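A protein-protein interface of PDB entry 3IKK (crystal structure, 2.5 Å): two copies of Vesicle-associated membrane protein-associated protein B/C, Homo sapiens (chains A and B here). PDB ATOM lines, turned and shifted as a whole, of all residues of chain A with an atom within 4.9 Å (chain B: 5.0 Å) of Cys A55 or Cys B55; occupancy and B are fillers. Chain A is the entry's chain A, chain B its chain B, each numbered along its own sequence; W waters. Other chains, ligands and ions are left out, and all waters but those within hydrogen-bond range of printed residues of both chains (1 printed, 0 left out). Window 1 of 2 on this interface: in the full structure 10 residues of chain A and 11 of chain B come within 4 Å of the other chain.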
ATOM      1  N   ARG A  53       2.600 -25.368  30.988  1.00  0.00           N
ATOM      2  CA  ARG A  53       1.899 -26.560  30.500  1.00  0.00           C
ATOM      3  C   ARG A  53       1.457 -26.498  29.029  1.00  0.00           C
ATOM      4  O   ARG A  53       1.291 -27.530  28.380  1.00  0.00           O
ATOM      5  CB  ARG A  53       0.653 -26.766  31.343  1.00  0.00           C
ATOM      6  CG  ARG A  53       0.928 -27.096  32.788  1.00  0.00           C
ATOM      7  CD  ARG A  53       1.129 -28.579  32.934  1.00  0.00           C
ATOM      8  NE  ARG A  53       0.099 -29.340  32.218  1.00  0.00           N
ATOM      9  CZ  ARG A  53      -0.811 -30.106  32.810  1.00  0.00           C
ATOM     10  NH1 ARG A  53      -0.824 -30.214  34.127  1.00  0.00           N
ATOM     11  NH2 ARG A  53      -1.694 -30.780  32.092  1.00  0.00           N
ATOM     12  N   TYR A  54       1.243 -25.291  28.520  1.00  0.00           N
ATOM     13  CA  TYR A  54       0.707 -25.105  27.184  1.00  0.00           C
ATOM     14  C   TYR A  54       1.662 -24.270  26.352  1.00  0.00           C
ATOM     15  O   TYR A  54       2.601 -23.678  26.886  1.00  0.00           O
ATOM     16  CB  TYR A  54      -0.649 -24.400  27.242  1.00  0.00           C
ATOM     17  CG  TYR A  54      -1.779 -25.251  27.770  1.00  0.00           C
ATOM     18  CD1 TYR A  54      -2.467 -26.123  26.939  1.00  0.00           C
ATOM     19  CD2 TYR A  54      -2.172 -25.166  29.094  1.00  0.00           C
ATOM     20  CE1 TYR A  54      -3.514 -26.899  27.424  1.00  0.00           C
ATOM     21  CE2 TYR A  54      -3.210 -25.922  29.575  1.00  0.00           C
ATOM     22  CZ  TYR A  54      -3.879 -26.792  28.742  1.00  0.00           C
ATOM     23  OH  TYR A  54      -4.909 -27.558  29.249  1.00  0.00           O
ATOM     24  N   CYS A  55       1.421 -24.246  25.043  1.00  0.00           N
ATOM     25  CA  CYS A  55       2.053 -23.293  24.135  1.00  0.00           C
ATOM     26  C   CYS A  55       1.065 -22.970  23.042  1.00  0.00           C
ATOM     27  O   CYS A  55       0.407 -23.867  22.508  1.00  0.00           O
ATOM     28  CB  CYS A  55       3.340 -23.848  23.515  1.00  0.00           C
ATOM     29  SG  CYS A  55       3.889 -22.924  22.031  1.00  0.00           S
ATOM     30  N   VAL A  56       0.961 -21.696  22.702  1.00  0.00           N
ATOM     31  CA  VAL A  56       0.015 -21.272  21.687  1.00  0.00           C
ATOM     32  C   VAL A  56       0.735 -20.694  20.459  1.00  0.00           C
ATOM     33  O   VAL A  56       1.547 -19.784  20.575  1.00  0.00           O
ATOM     34  CB  VAL A  56      -0.932 -20.210  22.260  1.00  0.00           C
ATOM     35  CG1 VAL A  56      -1.965 -19.817  21.221  1.00  0.00           C
ATOM     36  CG2 VAL A  56      -1.586 -20.700  23.541  1.00  0.00           C
ATOM     37  N   ARG A  57       0.430 -21.224  19.283  1.00  0.00           N
ATOM     38  CA  ARG A  57       0.989 -20.696  18.034  1.00  0.00           C
ATOM     39  C   ARG A  57      -0.100 -20.518  16.952  1.00  0.00           C
ATOM     40  O   ARG A  57      -0.608 -21.505  16.419  1.00  0.00           O
ATOM     41  CB  ARG A  57       2.132 -21.599  17.528  1.00  0.00           C
ATOM     42  CG  ARG A  57       3.400 -21.563  18.393  1.00  0.00           C
ATOM     43  CD  ARG A  57       3.886 -20.134  18.650  1.00  0.00           C
ATOM     44  NE  ARG A  57       5.340 -20.004  18.757  1.00  0.00           N
ATOM     45  CZ  ARG A  57       6.009 -19.867  19.900  1.00  0.00           C
ATOM     46  NH1 ARG A  57       7.335 -19.735  19.889  1.00  0.00           N
ATOM     47  NH2 ARG A  57       5.358 -19.851  21.059  1.00  0.00           N
ATOM     48  N   SER A  72      -2.824 -23.094  16.933  1.00  0.00           N
ATOM     49  CA  SER A  72      -2.450 -24.354  17.544  1.00  0.00           C
ATOM     50  C   SER A  72      -2.303 -24.222  19.055  1.00  0.00           C
ATOM     51  O   SER A  72      -1.456 -23.485  19.530  1.00  0.00           O
ATOM     52  CB  SER A  72      -1.155 -24.879  16.916  1.00  0.00           C
ATOM     53  OG  SER A  72      -1.386 -25.251  15.563  1.00  0.00           O
ATOM     54  N   VAL A  73      -3.143 -24.936  19.800  1.00  0.00           N
ATOM     55  CA  VAL A  73      -2.971 -25.082  21.251  1.00  0.00           C
ATOM     56  C   VAL A  73      -2.406 -26.463  21.615  1.00  0.00           C
ATOM     57  O   VAL A  73      -2.980 -27.504  21.282  1.00  0.00           O
ATOM     58  CB  VAL A  73      -4.266 -24.779  22.026  1.00  0.00           C
ATOM     59  CG1 VAL A  73      -4.164 -25.273  23.446  1.00  0.00           C
ATOM     60  CG2 VAL A  73      -4.560 -23.278  22.007  1.00  0.00           C
ATOM     61  N   MET A  74      -1.261 -26.444  22.294  1.00  0.00           N
ATOM     62  CA  MET A  74      -0.407 -27.613  22.422  1.00  0.00           C
ATOM     63  C   MET A  74      -0.129 -27.934  23.884  1.00  0.00           C
ATOM     64  O   MET A  74       0.369 -27.075  24.632  1.00  0.00           O
ATOM     65  CB  MET A  74       0.915 -27.364  21.688  1.00  0.00           C
ATOM     66  CG  MET A  74       0.747 -26.997  20.208  1.00  0.00           C
ATOM     67  SD  MET A  74       2.271 -26.470  19.356  1.00  0.00           S
ATOM     68  CE  MET A  74       2.410 -24.750  19.814  1.00  0.00           C
ATOM     69  N   ARG B  53       7.708 -20.216  13.895  1.00  0.00           N
ATOM     70  CA  ARG B  53       7.618 -21.567  13.328  1.00  0.00           C
ATOM     71  C   ARG B  53       7.700 -22.653  14.402  1.00  0.00           C
ATOM     72  O   ARG B  53       7.070 -23.715  14.282  1.00  0.00           O
ATOM     73  CB  ARG B  53       8.724 -21.805  12.288  1.00  0.00           C
ATOM     74  CG  ARG B  53       8.554 -21.049  10.971  1.00  0.00           C
ATOM     75  CD  ARG B  53       7.543 -21.733  10.080  1.00  0.00           C
ATOM     76  NE  ARG B  53       7.876 -23.147   9.915  1.00  0.00           N
ATOM     77  CZ  ARG B  53       8.379 -23.689   8.805  1.00  0.00           C
ATOM     78  NH1 ARG B  53       8.611 -22.945   7.724  1.00  0.00           N
ATOM     79  NH2 ARG B  53       8.639 -24.991   8.778  1.00  0.00           N
ATOM     80  N   TYR B  54       8.478 -22.392  15.450  1.00  0.00           N
ATOM     81  CA  TYR B  54       8.664 -23.369  16.516  1.00  0.00           C
ATOM     82  C   TYR B  54       8.122 -22.896  17.846  1.00  0.00           C
ATOM     83  O   TYR B  54       7.872 -21.708  18.032  1.00  0.00           O
ATOM     84  CB  TYR B  54      10.144 -23.666  16.696  1.00  0.00           C
ATOM     85  CG  TYR B  54      10.765 -24.342  15.524  1.00  0.00           C
ATOM     86  CD1 TYR B  54      10.759 -25.725  15.415  1.00  0.00           C
ATOM     87  CD2 TYR B  54      11.370 -23.607  14.521  1.00  0.00           C
ATOM     88  CE1 TYR B  54      11.345 -26.356  14.330  1.00  0.00           C
ATOM     89  CE2 TYR B  54      11.956 -24.226  13.432  1.00  0.00           C
ATOM     90  CZ  TYR B  54      11.938 -25.599  13.340  1.00  0.00           C
ATOM     91  OH  TYR B  54      12.518 -26.216  12.261  1.00  0.00           O
ATOM     92  N   CYS B  55       7.965 -23.842  18.771  1.00  0.00           N
ATOM     93  CA  CYS B  55       7.784 -23.535  20.179  1.00  0.00           C
ATOM     94  C   CYS B  55       8.759 -24.369  21.018  1.00  0.00           C
ATOM     95  O   CYS B  55       9.200 -25.447  20.597  1.00  0.00           O
ATOM     96  CB  CYS B  55       6.334 -23.780  20.606  1.00  0.00           C
ATOM     97  SG  CYS B  55       5.892 -23.176  22.289  1.00  0.00           S
ATOM     98  N   VAL B  56       9.112 -23.869  22.198  1.00  0.00           N
ATOM     99  CA  VAL B  56      10.050 -24.586  23.049  1.00  0.00           C
ATOM    100  C   VAL B  56       9.578 -24.587  24.468  1.00  0.00           C
ATOM    101  O   VAL B  56       9.733 -23.588  25.162  1.00  0.00           O
ATOM    102  CB  VAL B  56      11.450 -23.959  23.038  1.00  0.00           C
ATOM    103  CG1 VAL B  56      12.393 -24.778  23.916  1.00  0.00           C
ATOM    104  CG2 VAL B  56      11.967 -23.902  21.634  1.00  0.00           C
ATOM    105  N   ARG B  57       8.998 -25.715  24.877  1.00  0.00           N
ATOM    106  CA  ARG B  57       8.637 -25.980  26.257  1.00  0.00           C
ATOM    107  C   ARG B  57       9.616 -27.007  26.878  1.00  0.00           C
ATOM    108  O   ARG B  57       9.566 -28.191  26.569  1.00  0.00           O
ATOM    109  CB  ARG B  57       7.208 -26.529  26.332  1.00  0.00           C
ATOM    110  CG  ARG B  57       6.082 -25.523  26.136  1.00  0.00           C
ATOM    111  CD  ARG B  57       6.238 -24.243  26.972  1.00  0.00           C
ATOM    112  NE  ARG B  57       6.814 -23.139  26.199  1.00  0.00           N
ATOM    113  CZ  ARG B  57       6.151 -22.036  25.855  1.00  0.00           C
ATOM    114  NH1 ARG B  57       4.885 -21.877  26.213  1.00  0.00           N
ATOM    115  NH2 ARG B  57       6.752 -21.074  25.168  1.00  0.00           N
ATOM    116  N   SER B  72      10.689 -30.440  24.959  1.00  0.00           N
ATOM    117  CA  SER B  72       9.785 -30.567  23.808  1.00  0.00           C
ATOM    118  C   SER B  72       9.987 -29.430  22.808  1.00  0.00           C
ATOM    119  O   SER B  72       9.826 -28.263  23.158  1.00  0.00           O
ATOM    120  CB  SER B  72       8.327 -30.574  24.270  1.00  0.00           C
ATOM    121  OG  SER B  72       8.108 -31.557  25.272  1.00  0.00           O
ATOM    122  N   VAL B  73      10.343 -29.777  21.571  1.00  0.00           N
ATOM    123  CA  VAL B  73      10.534 -28.806  20.488  1.00  0.00           C
ATOM    124  C   VAL B  73       9.501 -29.034  19.393  1.00  0.00           C
ATOM    125  O   VAL B  73       9.600 -29.982  18.607  1.00  0.00           O
ATOM    126  CB  VAL B  73      11.963 -28.861  19.885  1.00  0.00           C
ATOM    127  CG1 VAL B  73      12.036 -28.091  18.568  1.00  0.00           C
ATOM    128  CG2 VAL B  73      12.984 -28.304  20.875  1.00  0.00           C
ATOM    129  N   MET B  74       8.516 -28.143  19.339  1.00  0.00           N
ATOM    130  CA  MET B  74       7.325 -28.345  18.516  1.00  0.00           C
ATOM    131  C   MET B  74       7.284 -27.520  17.226  1.00  0.00           C
ATOM    132  O   MET B  74       7.425 -26.303  17.241  1.00  0.00           O
ATOM    133  CB  MET B  74       6.100 -28.063  19.361  1.00  0.00           C
ATOM    134  CG  MET B  74       6.211 -28.751  20.705  1.00  0.00           C
ATOM    135  SD  MET B  74       5.160 -28.061  21.975  1.00  0.00           S
ATOM    136  CE  MET B  74       6.084 -26.572  22.365  1.00  0.00           C
HETATM  137  O   HOH W   1       9.045 -20.809  21.720  1.00  0.00           O
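SG of Cys B55 is in hydrogen-bond range of NH2 of Arg A57 (3.6 Å). O of Tyr B54 is in hydrogen-bond range of NH1 of Arg A57 (2.8 Å). SG of Cys A55 is disulfide-bonded to SG of Cys B55, at 2.0 Å. The guanidinium group (NH1) of Arg B57 lies within hydrogen-bond range of the backbone carbonyl oxygen (O) of Tyr A54 (3.0 Å).
Of chain B, only Cys B55 and Arg B57 come within 4 Å of Cys A55. Cys B55 touches just these residues of chain A: Cys A55 and Arg A57. Of the printed residues of chain B, Arg A57 touches Tyr B54 (2.8 Å) and Cys B55 (3.6 Å). Printed residues of chain B within 4 Å of Tyr A54: Arg B57. Of the printed residues of chain A, Tyr B54 touches Arg A57. Val B56 touches none of the printed residues of chain A. Val B73 touches none of the printed residues of chain A. The nearest residue of chain B that does not touch Cys A55 is Met B74 (4.03 Å). The nearest residue of chain A that does not touch Cys B55 is Met A74 (4.1 Å).
Tyr A54 touches Arg B57, and with the chains exchanged Arg A57 touches Tyr B54. Cys A55 touches its own counterpart, Cys B55. Cys A55 touches Arg B57, and with the chains exchanged Arg A57 touches Cys B55. Positions printed for both chains: 53, 54, 55, 56, 57, 72, 73 and 74. Of the 5 pairs that touch across the chains among the printed residues, 5 have their exchanged pair printed and touching as well.
Among the printed residues, pairs that only touch across the chains: Cys A55 with Arg B57 (3.7 Å).
Water W1 lies within hydrogen-bond range of NH1 of Arg A57 (2.7 Å) and N of Val B56 (3.1 Å).
The side-chain sulfur (SG) of Cys A55 lies within hydrogen-bond range of the guanidinium group (NH2) of Arg A57. O of Arg B57 is in hydrogen-bond range of N of Ser B72 (3.0 Å). The side-chain sulfur of Cys B55 sits at hydrogen-bond distance from the guanidinium group of Arg B57 (3.7 Å). N of Cys B55 lies within hydrogen-bond range of O of Met B74, 2.9 Å away. N of Cys A55 is in hydrogen-bond range of O of Met A74. The backbone NH of Ser A72 sits at hydrogen-bond distance from the backbone carbonyl oxygen of Arg A57 (2.8 Å).
Of the 8 printed residues of chain B, 3 touch a printed residue of chain A. Printed residues of chain B that touch a printed residue of chain A: Tyr B54, Cys B55 and Arg B57. Among the printed residues, no Asp or Glu carboxylate lies within 4 Å of a Lys or Arg side-chain nitrogen of the other chain.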
